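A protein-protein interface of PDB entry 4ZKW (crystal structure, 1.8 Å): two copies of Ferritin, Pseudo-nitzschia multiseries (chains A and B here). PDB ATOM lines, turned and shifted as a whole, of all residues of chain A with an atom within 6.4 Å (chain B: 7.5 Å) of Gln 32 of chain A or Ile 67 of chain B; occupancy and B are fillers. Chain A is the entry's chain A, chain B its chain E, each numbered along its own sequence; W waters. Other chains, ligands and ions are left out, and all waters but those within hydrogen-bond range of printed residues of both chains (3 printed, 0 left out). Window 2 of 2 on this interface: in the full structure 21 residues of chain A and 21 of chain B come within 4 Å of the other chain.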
ATOM      1  N   SER A  25      -8.397   6.206  17.488  1.00  0.00           N
ATOM      2  CA  SER A  25      -7.319   6.169  16.478  1.00  0.00           C
ATOM      3  C   SER A  25      -7.806   6.586  15.083  1.00  0.00           C
ATOM      4  O   SER A  25      -7.096   7.229  14.325  1.00  0.00           O
ATOM      5  CB  SER A  25      -6.642   4.798  16.420  1.00  0.00           C
ATOM      6  OG  SER A  25      -7.499   3.820  15.826  1.00  0.00           O
ATOM      7  N   SER A  27     -10.205   8.832  14.602  1.00  0.00           N
ATOM      8  CA  SER A  27     -10.297  10.306  14.742  1.00  0.00           C
ATOM      9  C   SER A  27      -8.981  11.018  14.554  1.00  0.00           C
ATOM     10  O   SER A  27      -8.845  12.096  13.949  1.00  0.00           O
ATOM     11  CB  SER A  27     -10.912  10.714  16.112  1.00  0.00           C
ATOM     12  OG  SER A  27      -9.945  10.909  17.161  1.00  0.00           O
ATOM     13  N   ILE A  28      -7.958  10.425  15.103  1.00  0.00           N
ATOM     14  CA  ILE A  28      -6.690  10.989  14.999  1.00  0.00           C
ATOM     15  C   ILE A  28      -6.186  10.992  13.571  1.00  0.00           C
ATOM     16  O   ILE A  28      -5.642  11.979  13.112  1.00  0.00           O
ATOM     17  CB  ILE A  28      -5.709  10.238  15.947  1.00  0.00           C
ATOM     18  CG1 ILE A  28      -6.075  10.510  17.400  1.00  0.00           C
ATOM     19  CG2 ILE A  28      -4.302  10.644  15.673  1.00  0.00           C
ATOM     20  CD1 ILE A  28      -5.389   9.595  18.455  1.00  0.00           C
ATOM     21  N   TRP A  29      -6.313   9.877  12.876  1.00  0.00           N
ATOM     22  CA  TRP A  29      -5.804   9.806  11.526  1.00  0.00           C
ATOM     23  C   TRP A  29      -6.595  10.819  10.739  1.00  0.00           C
ATOM     24  O   TRP A  29      -6.026  11.525   9.917  1.00  0.00           O
ATOM     25  CB  TRP A  29      -6.063   8.415  10.929  1.00  0.00           C
ATOM     26  CG  TRP A  29      -5.440   8.289   9.613  1.00  0.00           C
ATOM     27  CD1 TRP A  29      -4.180   7.774   9.350  1.00  0.00           C
ATOM     28  CD2 TRP A  29      -5.994   8.624   8.347  1.00  0.00           C
ATOM     29  NE1 TRP A  29      -3.903   7.855   8.028  1.00  0.00           N
ATOM     30  CE2 TRP A  29      -4.995   8.346   7.373  1.00  0.00           C
ATOM     31  CE3 TRP A  29      -7.190   9.217   7.926  1.00  0.00           C
ATOM     32  CZ2 TRP A  29      -5.198   8.587   6.026  1.00  0.00           C
ATOM     33  CZ3 TRP A  29      -7.375   9.466   6.592  1.00  0.00           C
ATOM     34  CH2 TRP A  29      -6.412   9.150   5.653  1.00  0.00           C
ATOM     35  N   PHE A  30      -7.887  10.884  10.980  1.00  0.00           N
ATOM     36  CA  PHE A  30      -8.690  11.858  10.158  1.00  0.00           C
ATOM     37  C   PHE A  30      -8.260  13.287  10.449  1.00  0.00           C
ATOM     38  O   PHE A  30      -8.030  14.064   9.532  1.00  0.00           O
ATOM     39  CB  PHE A  30     -10.141  11.692  10.398  1.00  0.00           C
ATOM     40  CG  PHE A  30     -10.760  10.524   9.665  1.00  0.00           C
ATOM     41  CD1 PHE A  30     -10.583  10.372   8.283  1.00  0.00           C
ATOM     42  CD2 PHE A  30     -11.618   9.662  10.310  1.00  0.00           C
ATOM     43  CE1 PHE A  30     -11.204   9.356   7.613  1.00  0.00           C
ATOM     44  CE2 PHE A  30     -12.190   8.615   9.645  1.00  0.00           C
ATOM     45  CZ  PHE A  30     -11.982   8.442   8.281  1.00  0.00           C
ATOM     46  N   ASP A  31      -8.193  13.638  11.710  1.00  0.00           N
ATOM     47  CA  ASP A  31      -7.718  14.997  12.102  1.00  0.00           C
ATOM     48  C   ASP A  31      -6.339  15.339  11.553  1.00  0.00           C
ATOM     49  O   ASP A  31      -6.095  16.424  11.013  1.00  0.00           O
ATOM     50  CB  ASP A  31      -7.700  15.141  13.620  1.00  0.00           C
ATOM     51  CG  ASP A  31      -9.021  15.672  14.189  1.00  0.00           C
ATOM     52  OD1 ASP A  31      -9.639  16.544  13.484  1.00  0.00           O
ATOM     53  OD2 ASP A  31      -9.463  15.200  15.292  1.00  0.00           O
ATOM     54  N   GLN A  32      -5.404  14.379  11.630  1.00  0.00           N
ATOM     55  CA  GLN A  32      -4.041  14.643  11.153  1.00  0.00           C
ATOM     56  C   GLN A  32      -4.039  14.902   9.684  1.00  0.00           C
ATOM     57  O   GLN A  32      -3.114  15.524   9.239  1.00  0.00           O
ATOM     58  CB  GLN A  32      -3.035  13.478  11.435  1.00  0.00           C
ATOM     59  CG  GLN A  32      -2.746  13.172  12.908  1.00  0.00           C
ATOM     60  CD  GLN A  32      -2.036  11.763  13.172  1.00  0.00           C
ATOM     61  OE1 GLN A  32      -2.168  10.770  12.389  1.00  0.00           O
ATOM     62  NE2 GLN A  32      -1.344  11.672  14.319  1.00  0.00           N
ATOM     63  N   ASN A  33      -5.017  14.345   8.956  1.00  0.00           N
ATOM     64  CA  ASN A  33      -5.137  14.406   7.513  1.00  0.00           C
ATOM     65  C   ASN A  33      -6.242  15.360   6.997  1.00  0.00           C
ATOM     66  O   ASN A  33      -6.585  15.350   5.828  1.00  0.00           O
ATOM     67  CB  ASN A  33      -5.267  13.032   6.931  1.00  0.00           C
ATOM     68  CG  ASN A  33      -3.989  12.253   7.069  1.00  0.00           C
ATOM     69  OD1 ASN A  33      -3.111  12.402   6.260  1.00  0.00           O
ATOM     70  ND2 ASN A  33      -3.876  11.447   8.076  1.00  0.00           N
ATOM     71  N   ASP A  34      -6.660  16.226   7.892  1.00  0.00           N
ATOM     72  CA  ASP A  34      -7.568  17.341   7.672  1.00  0.00           C
ATOM     73  C   ASP A  34      -8.949  16.922   7.201  1.00  0.00           C
ATOM     74  O   ASP A  34      -9.566  17.595   6.396  1.00  0.00           O
ATOM     75  CB  ASP A  34      -6.886  18.377   6.821  1.00  0.00           C
ATOM     76  CG  ASP A  34      -5.566  18.822   7.404  1.00  0.00           C
ATOM     77  OD1 ASP A  34      -5.475  19.391   8.544  1.00  0.00           O
ATOM     78  OD2 ASP A  34      -4.610  18.651   6.685  1.00  0.00           O
ATOM     79  N   TRP A  35      -9.442  15.811   7.744  1.00  0.00           N
ATOM     80  CA  TRP A  35     -10.797  15.320   7.528  1.00  0.00           C
ATOM     81  C   TRP A  35     -11.568  15.542   8.848  1.00  0.00           C
ATOM     82  O   TRP A  35     -11.978  14.551   9.572  1.00  0.00           O
ATOM     83  CB  TRP A  35     -10.806  13.847   7.127  1.00  0.00           C
ATOM     84  CG  TRP A  35     -10.120  13.519   5.927  1.00  0.00           C
ATOM     85  CD1 TRP A  35      -8.817  13.166   5.794  1.00  0.00           C
ATOM     86  CD2 TRP A  35     -10.683  13.500   4.631  1.00  0.00           C
ATOM     87  NE1 TRP A  35      -8.533  12.906   4.483  1.00  0.00           N
ATOM     88  CE2 TRP A  35      -9.659  13.126   3.741  1.00  0.00           C
ATOM     89  CE3 TRP A  35     -11.955  13.781   4.139  1.00  0.00           C
ATOM     90  CZ2 TRP A  35      -9.861  13.046   2.370  1.00  0.00           C
ATOM     91  CZ3 TRP A  35     -12.177  13.653   2.795  1.00  0.00           C
ATOM     92  CH2 TRP A  35     -11.134  13.317   1.924  1.00  0.00           C
ATOM     93  N   YCM A  78      -4.140   1.678  12.361  1.00  0.00           N
ATOM     94  CA  YCM A  78      -3.669   3.025  12.071  1.00  0.00           C
ATOM     95  CB  YCM A  78      -3.289   3.761  13.321  1.00  0.00           C
ATOM     96  SG  YCM A  78      -3.891   5.311  12.990  1.00  0.00           S
ATOM     97  CD  YCM A  78      -2.680   6.268  12.450  1.00  0.00           C
ATOM     98  CE  YCM A  78      -3.035   7.487  13.206  1.00  0.00           C
ATOM     99  OZ1 YCM A  78      -2.563   8.564  12.864  1.00  0.00           O
ATOM    100  NZ2 YCM A  78      -3.905   7.308  14.296  1.00  0.00           N
ATOM    101  C   YCM A  78      -2.462   3.124  11.241  1.00  0.00           C
ATOM    102  O   YCM A  78      -2.393   3.926  10.320  1.00  0.00           O
ATOM    103  N   LEU B   6       8.219  15.422  22.119  1.00  0.00           N
ATOM    104  CA  LEU B   6       7.257  14.526  21.467  1.00  0.00           C
ATOM    105  C   LEU B   6       6.943  13.247  22.239  1.00  0.00           C
ATOM    106  O   LEU B   6       5.780  12.859  22.364  1.00  0.00           O
ATOM    107  CB  LEU B   6       7.682  14.011  20.072  1.00  0.00           C
ATOM    108  CG  LEU B   6       6.960  12.690  19.573  1.00  0.00           C
ATOM    109  CD1 LEU B   6       5.446  12.883  19.384  1.00  0.00           C
ATOM    110  CD2 LEU B   6       7.477  11.980  18.301  1.00  0.00           C
ATOM    111  N   PHE B   9       5.026  13.961  25.391  1.00  0.00           N
ATOM    112  CA  PHE B   9       3.706  14.418  25.108  1.00  0.00           C
ATOM    113  C   PHE B   9       2.840  13.184  24.870  1.00  0.00           C
ATOM    114  O   PHE B   9       1.733  13.057  25.431  1.00  0.00           O
ATOM    115  CB  PHE B   9       3.726  15.487  23.977  1.00  0.00           C
ATOM    116  CG  PHE B   9       2.506  16.376  23.979  1.00  0.00           C
ATOM    117  CD1 PHE B   9       1.344  15.866  23.549  1.00  0.00           C
ATOM    118  CD2 PHE B   9       2.525  17.685  24.449  1.00  0.00           C
ATOM    119  CE1 PHE B   9       0.167  16.566  23.604  1.00  0.00           C
ATOM    120  CE2 PHE B   9       1.352  18.421  24.433  1.00  0.00           C
ATOM    121  CZ  PHE B   9       0.177  17.840  24.015  1.00  0.00           C
ATOM    122  N   ASN B  10       3.342  12.171  24.126  1.00  0.00           N
ATOM    123  CA  ASN B  10       2.626  10.913  23.995  1.00  0.00           C
ATOM    124  C   ASN B  10       2.403  10.138  25.242  1.00  0.00           C
ATOM    125  O   ASN B  10       1.369   9.534  25.412  1.00  0.00           O
ATOM    126  CB  ASN B  10       3.314   9.885  23.100  1.00  0.00           C
ATOM    127  CG  ASN B  10       2.924  10.041  21.684  1.00  0.00           C
ATOM    128  OD1 ASN B  10       1.972   9.414  21.208  1.00  0.00           O
ATOM    129  ND2 ASN B  10       3.611  10.994  21.017  1.00  0.00           N
ATOM    130  N   ARG B  11       3.396  10.113  26.087  1.00  0.00           N
ATOM    131  CA  ARG B  11       3.275   9.431  27.349  1.00  0.00           C
ATOM    132  C   ARG B  11       2.260  10.070  28.258  1.00  0.00           C
ATOM    133  O   ARG B  11       1.607   9.390  29.059  1.00  0.00           O
ATOM    134  CB  ARG B  11       4.626   9.307  28.014  1.00  0.00           C
ATOM    135  CG  ARG B  11       5.441   8.296  27.196  1.00  0.00           C
ATOM    136  CD  ARG B  11       6.478   7.533  27.980  1.00  0.00           C
ATOM    137  NE  ARG B  11       7.636   8.357  28.253  1.00  0.00           N
ATOM    138  CZ  ARG B  11       8.801   7.887  28.679  1.00  0.00           C
ATOM    139  NH1 ARG B  11       8.980   6.576  28.899  1.00  0.00           N
ATOM    140  NH2 ARG B  11       9.785   8.738  28.901  1.00  0.00           N
ATOM    141  N   VAL B  13      -0.632  11.467  27.206  1.00  0.00           N
ATOM    142  CA  VAL B  13      -1.853  10.848  26.730  1.00  0.00           C
ATOM    143  C   VAL B  13      -2.102   9.487  27.377  1.00  0.00           C
ATOM    144  O   VAL B  13      -3.155   9.213  27.988  1.00  0.00           O
ATOM    145  CB  VAL B  13      -1.942  10.774  25.197  1.00  0.00           C
ATOM    146  CG1 VAL B  13      -3.165  10.017  24.774  1.00  0.00           C
ATOM    147  CG2 VAL B  13      -1.871  12.189  24.614  1.00  0.00           C
ATOM    148  N   THR B  14      -1.090   8.611  27.273  1.00  0.00           N
ATOM    149  CA  THR B  14      -1.154   7.327  27.963  1.00  0.00           C
ATOM    150  C   THR B  14      -1.422   7.464  29.482  1.00  0.00           C
ATOM    151  O   THR B  14      -2.252   6.699  30.024  1.00  0.00           O
ATOM    152  CB  THR B  14       0.165   6.551  27.742  1.00  0.00           C
ATOM    153  OG1 THR B  14       0.380   6.477  26.323  1.00  0.00           O
ATOM    154  CG2 THR B  14       0.058   5.166  28.357  1.00  0.00           C
ATOM    155  N   PHE B  17      -5.176   8.274  30.095  1.00  0.00           N
ATOM    156  CA  PHE B  17      -6.070   7.167  29.860  1.00  0.00           C
ATOM    157  C   PHE B  17      -5.874   6.009  30.884  1.00  0.00           C
ATOM    158  O   PHE B  17      -6.793   5.309  31.230  1.00  0.00           O
ATOM    159  CB  PHE B  17      -5.915   6.666  28.453  1.00  0.00           C
ATOM    160  CG  PHE B  17      -6.397   7.647  27.382  1.00  0.00           C
ATOM    161  CD1 PHE B  17      -7.325   8.628  27.647  1.00  0.00           C
ATOM    162  CD2 PHE B  17      -5.925   7.554  26.109  1.00  0.00           C
ATOM    163  CE1 PHE B  17      -7.793   9.460  26.652  1.00  0.00           C
ATOM    164  CE2 PHE B  17      -6.314   8.460  25.130  1.00  0.00           C
ATOM    165  CZ  PHE B  17      -7.271   9.408  25.399  1.00  0.00           C
ATOM    166  N   GLY B  53      -7.140  13.485  28.623  1.00  0.00           N
ATOM    167  CA  GLY B  53      -6.445  12.791  27.562  1.00  0.00           C
ATOM    168  C   GLY B  53      -6.846  13.297  26.153  1.00  0.00           C
ATOM    169  O   GLY B  53      -5.959  13.513  25.260  1.00  0.00           O
ATOM    170  N   PHE B  56      -5.388  16.670  25.377  1.00  0.00           N
ATOM    171  CA  PHE B  56      -3.998  16.478  24.906  1.00  0.00           C
ATOM    172  C   PHE B  56      -3.864  15.967  23.472  1.00  0.00           C
ATOM    173  O   PHE B  56      -3.057  16.514  22.702  1.00  0.00           O
ATOM    174  CB  PHE B  56      -3.191  15.560  25.827  1.00  0.00           C
ATOM    175  CG  PHE B  56      -2.613  16.298  27.012  1.00  0.00           C
ATOM    176  CD1 PHE B  56      -3.409  16.615  28.089  1.00  0.00           C
ATOM    177  CD2 PHE B  56      -1.290  16.621  27.053  1.00  0.00           C
ATOM    178  CE1 PHE B  56      -2.906  17.286  29.174  1.00  0.00           C
ATOM    179  CE2 PHE B  56      -0.761  17.292  28.153  1.00  0.00           C
ATOM    180  CZ  PHE B  56      -1.586  17.633  29.218  1.00  0.00           C
ATOM    181  N   VAL B  57      -4.708  14.995  23.095  1.00  0.00           N
ATOM    182  CA  VAL B  57      -4.733  14.518  21.720  1.00  0.00           C
ATOM    183  C   VAL B  57      -5.086  15.658  20.766  1.00  0.00           C
ATOM    184  O   VAL B  57      -4.420  15.813  19.744  1.00  0.00           O
ATOM    185  CB  VAL B  57      -5.714  13.365  21.585  1.00  0.00           C
ATOM    186  CG1 VAL B  57      -6.007  12.981  20.134  1.00  0.00           C
ATOM    187  CG2 VAL B  57      -5.113  12.160  22.337  1.00  0.00           C
ATOM    188  N   ASP B  58      -6.076  16.473  21.134  1.00  0.00           N
ATOM    189  CA  ASP B  58      -6.538  17.548  20.270  1.00  0.00           C
ATOM    190  C   ASP B  58      -5.438  18.564  20.035  1.00  0.00           C
ATOM    191  O   ASP B  58      -5.158  18.925  18.864  1.00  0.00           O
ATOM    192  CB  ASP B  58      -7.792  18.142  20.845  1.00  0.00           C
ATOM    193  CG  ASP B  58      -8.385  19.294  19.942  1.00  0.00           C
ATOM    194  OD1 ASP B  58      -8.470  19.127  18.763  1.00  0.00           O
ATOM    195  OD2 ASP B  58      -8.790  20.298  20.457  1.00  0.00           O
ATOM    196  N   PHE B  59      -4.761  18.974  21.100  1.00  0.00           N
ATOM    197  CA  PHE B  59      -3.672  19.920  20.935  1.00  0.00           C
ATOM    198  C   PHE B  59      -2.542  19.354  20.092  1.00  0.00           C
ATOM    199  O   PHE B  59      -1.950  20.017  19.216  1.00  0.00           O
ATOM    200  CB  PHE B  59      -3.148  20.311  22.282  1.00  0.00           C
ATOM    201  CG  PHE B  59      -2.048  21.306  22.231  1.00  0.00           C
ATOM    202  CD1 PHE B  59      -2.359  22.642  22.187  1.00  0.00           C
ATOM    203  CD2 PHE B  59      -0.742  20.921  22.248  1.00  0.00           C
ATOM    204  CE1 PHE B  59      -1.389  23.582  22.124  1.00  0.00           C
ATOM    205  CE2 PHE B  59       0.290  21.875  22.190  1.00  0.00           C
ATOM    206  CZ  PHE B  59      -0.055  23.193  22.098  1.00  0.00           C
ATOM    207  N   ALA B  60      -2.194  18.111  20.371  1.00  0.00           N
ATOM    208  CA  ALA B  60      -1.156  17.469  19.599  1.00  0.00           C
ATOM    209  C   ALA B  60      -1.476  17.442  18.115  1.00  0.00           C
ATOM    210  O   ALA B  60      -0.576  17.772  17.316  1.00  0.00           O
ATOM    211  CB  ALA B  60      -0.900  16.039  20.103  1.00  0.00           C
ATOM    212  N   ASN B  61      -2.685  17.044  17.766  1.00  0.00           N
ATOM    213  CA  ASN B  61      -3.127  17.016  16.371  1.00  0.00           C
ATOM    214  C   ASN B  61      -2.913  18.436  15.739  1.00  0.00           C
ATOM    215  O   ASN B  61      -2.357  18.581  14.622  1.00  0.00           O
ATOM    216  CB  ASN B  61      -4.571  16.638  16.253  1.00  0.00           C
ATOM    217  CG  ASN B  61      -4.840  15.132  16.575  1.00  0.00           C
ATOM    218  OD1 ASN B  61      -3.899  14.302  16.616  1.00  0.00           O
ATOM    219  ND2 ASN B  61      -6.106  14.809  16.854  1.00  0.00           N
ATOM    220  N   LYS B  62      -3.354  19.460  16.439  1.00  0.00           N
ATOM    221  CA  LYS B  62      -3.252  20.883  15.930  1.00  0.00           C
ATOM    222  C   LYS B  62      -1.826  21.340  15.733  1.00  0.00           C
ATOM    223  O   LYS B  62      -1.530  22.043  14.781  1.00  0.00           O
ATOM    224  CB  LYS B  62      -3.996  21.855  16.878  1.00  0.00           C
ATOM    225  CG  LYS B  62      -5.500  21.661  16.784  1.00  0.00           C
ATOM    226  CD  LYS B  62      -6.368  22.729  17.472  1.00  0.00           C
ATOM    227  CE  LYS B  62      -6.468  22.580  18.964  1.00  0.00           C
ATOM    228  NZ  LYS B  62      -7.352  23.619  19.585  1.00  0.00           N
ATOM    229  N   ASN B  64       0.805  19.390  15.194  1.00  0.00           N
ATOM    230  CA  ASN B  64       1.509  18.399  14.418  1.00  0.00           C
ATOM    231  C   ASN B  64       2.494  17.596  15.261  1.00  0.00           C
ATOM    232  O   ASN B  64       3.576  17.260  14.819  1.00  0.00           O
ATOM    233  CB  ASN B  64       2.201  19.046  13.201  1.00  0.00           C
ATOM    234  CG  ASN B  64       1.226  19.781  12.364  1.00  0.00           C
ATOM    235  OD1 ASN B  64       0.247  19.229  11.856  1.00  0.00           O
ATOM    236  ND2 ASN B  64       1.394  21.061  12.338  1.00  0.00           N
ATOM    237  N   ILE B  65       2.090  17.299  16.467  1.00  0.00           N
ATOM    238  CA  ILE B  65       2.797  16.343  17.372  1.00  0.00           C
ATOM    239  C   ILE B  65       2.176  14.987  17.092  1.00  0.00           C
ATOM    240  O   ILE B  65       0.985  14.781  17.389  1.00  0.00           O
ATOM    241  CB  ILE B  65       2.611  16.742  18.848  1.00  0.00           C
ATOM    242  CG1 ILE B  65       3.303  18.099  19.111  1.00  0.00           C
ATOM    243  CG2 ILE B  65       3.203  15.731  19.790  1.00  0.00           C
ATOM    244  CD1 ILE B  65       3.022  18.696  20.460  1.00  0.00           C
ATOM    245  N   PRO B  66       2.948  14.059  16.511  1.00  0.00           N
ATOM    246  CA  PRO B  66       2.368  12.768  16.132  1.00  0.00           C
ATOM    247  C   PRO B  66       1.925  11.985  17.390  1.00  0.00           C
ATOM    248  O   PRO B  66       2.649  11.930  18.402  1.00  0.00           O
ATOM    249  CB  PRO B  66       3.528  12.043  15.397  1.00  0.00           C
ATOM    250  CG  PRO B  66       4.774  12.837  15.702  1.00  0.00           C
ATOM    251  CD  PRO B  66       4.294  14.251  15.918  1.00  0.00           C
ATOM    252  N   ILE B  67       0.717  11.516  17.394  1.00  0.00           N
ATOM    253  CA  ILE B  67       0.264  10.745  18.571  1.00  0.00           C
ATOM    254  C   ILE B  67       0.156   9.308  18.064  1.00  0.00           C
ATOM    255  O   ILE B  67      -0.469   9.100  17.046  1.00  0.00           O
ATOM    256  CB  ILE B  67      -1.108  11.198  19.059  1.00  0.00           C
ATOM    257  CG1 ILE B  67      -1.045  12.586  19.724  1.00  0.00           C
ATOM    258  CG2 ILE B  67      -1.688  10.121  19.992  1.00  0.00           C
ATOM    259  CD1 ILE B  67      -0.155  12.653  20.962  1.00  0.00           C
ATOM    260  N   GLU B  68       0.751   8.383  18.797  1.00  0.00           N
ATOM    261  CA  GLU B  68       0.466   6.994  18.642  1.00  0.00           C
ATOM    262  C   GLU B  68      -0.081   6.407  19.984  1.00  0.00           C
ATOM    263  O   GLU B  68       0.605   6.472  20.972  1.00  0.00           O
ATOM    264  CB  GLU B  68       1.701   6.208  18.208  1.00  0.00           C
ATOM    265  CG  GLU B  68       1.197   5.024  17.396  1.00  0.00           C
ATOM    266  CD  GLU B  68       2.327   4.192  16.827  1.00  0.00           C
ATOM    267  OE1 GLU B  68       2.185   2.928  16.777  1.00  0.00           O
ATOM    268  OE2 GLU B  68       3.346   4.826  16.470  1.00  0.00           O
ATOM    269  N   LEU B  69      -1.346   6.006  19.922  1.00  0.00           N
ATOM    270  CA  LEU B  69      -2.055   5.474  21.069  1.00  0.00           C
ATOM    271  C   LEU B  69      -1.367   4.158  21.503  1.00  0.00           C
ATOM    272  O   LEU B  69      -1.215   3.263  20.688  1.00  0.00           O
ATOM    273  CB  LEU B  69      -3.512   5.249  20.748  1.00  0.00           C
ATOM    274  CG  LEU B  69      -4.340   6.558  20.549  1.00  0.00           C
ATOM    275  CD1 LEU B  69      -5.743   6.173  20.245  1.00  0.00           C
ATOM    276  CD2 LEU B  69      -4.205   7.473  21.759  1.00  0.00           C
ATOM    277  N   GLN B  70      -1.039   4.095  22.778  1.00  0.00           N
ATOM    278  CA  GLN B  70      -0.345   2.986  23.400  1.00  0.00           C
ATOM    279  C   GLN B  70      -1.390   2.156  24.120  1.00  0.00           C
ATOM    280  O   GLN B  70      -2.577   2.524  24.250  1.00  0.00           O
ATOM    281  CB  GLN B  70       0.734   3.494  24.337  1.00  0.00           C
ATOM    282  CG  GLN B  70       1.778   4.311  23.586  1.00  0.00           C
ATOM    283  CD  GLN B  70       2.804   3.442  22.877  1.00  0.00           C
ATOM    284  OE1 GLN B  70       3.510   2.656  23.516  1.00  0.00           O
ATOM    285  NE2 GLN B  70       2.899   3.586  21.564  1.00  0.00           N
HETATM  286  O   HOH W   1      -8.635  13.243  17.197  1.00  0.00           O
HETATM  287  O   HOH W   2      -1.238  14.009  16.103  1.00  0.00           O
HETATM  288  O   HOH W   3      -7.823  17.392  16.752  1.00  0.00           O
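Printed residues of chain B that touch a printed residue of chain A: Val 57, Asn 61, Ile 67 and Leu 69.
Hydrophobic or aromatic side chains of chain B within 4 Å of the printed part of chain A: Val 57 and Leu 69.
Among the printed residues, 6 pairs touch across the chains.
Among the printed residues, no Asp or Glu carboxylate lies within 4 Å of a Lys or Arg side-chain nitrogen of the other chain.
Gln 32 of chain A touches just one residue of chain B: Ile 67 (3.7 Å).
Ile 67 of chain B touches just one residue of chain A: Gln 32.
Of the printed residues of chain B, Asp 31 of chain A touches Asn 61.
Printed residues of chain A within 4 Å of Val 57 of chain B: Ile 28.
Of the printed residues of chain A, Asn 61 of chain B touches Ile 28 and Asp 31.
Of the printed residues of chain B, Ser 25 of chain A touches Leu 69.
Of the printed residues of chain A, Leu 69 of chain B touches Ser 25 and Ile 28.
Ile 65 of chain B touches none of the printed residues of chain A.
Arg 11 of chain B touches none of the printed residues of chain A.
The nearest printed residue of chain A that does not touch Leu 69 of chain B is YCM 78 of chain A (6.3 Å).
Among the printed residues, pairs that only touch across the chains: Ser 25 of chain A with Leu 69 of chain B, Ile 28 of chain A with Val 57 of chain B, Ile 28 of chain A with Asn 61 of chain B, Ile 28 of chain A with Leu 69 of chain B, Asp 31 of chain A with Asn 61 of chain B and Gln 32 of chain A with Ile 67 of chain B.
The backbone carbonyl oxygen of Ser 25 of chain A lies within hydrogen-bond range of NZ2 of YCM 78 of chain A, at 3.2 Å.
The side-chain amide nitrogen (ND2) of Asn 61 of chain B lies close to the backbone carbonyl oxygen (O) of Val 57 of chain B (3.5 Å).
No position is printed for both chains.
Of the 6 pairs that touch across the chains among the printed residues, none has its exchanged pair printed and touching as well.
Water W1 lies within hydrogen-bond range of OG of Ser 27 of chain A (2.7 Å), OD2 of Asp 31 of chain A (2.9 Å) and ND2 of Asn 61 of chain B (3.0 Å).
Water W2 lies within hydrogen-bond range of O of Ile 65 of chain B (2.7 Å), OD1 of Asn 61 of chain B (2.7 Å), NE2 of Gln 32 of chain A (2.9 Å) and N of Ile 67 of chain B (3.4 Å).
Water W3 lies within hydrogen-bond range of OD1 of Asp 58 of chain B (2.7 Å), OD2 of Asp 31 of chain A (3.1 Å) and ND2 of Asn 61 of chain B (3.1 Å).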
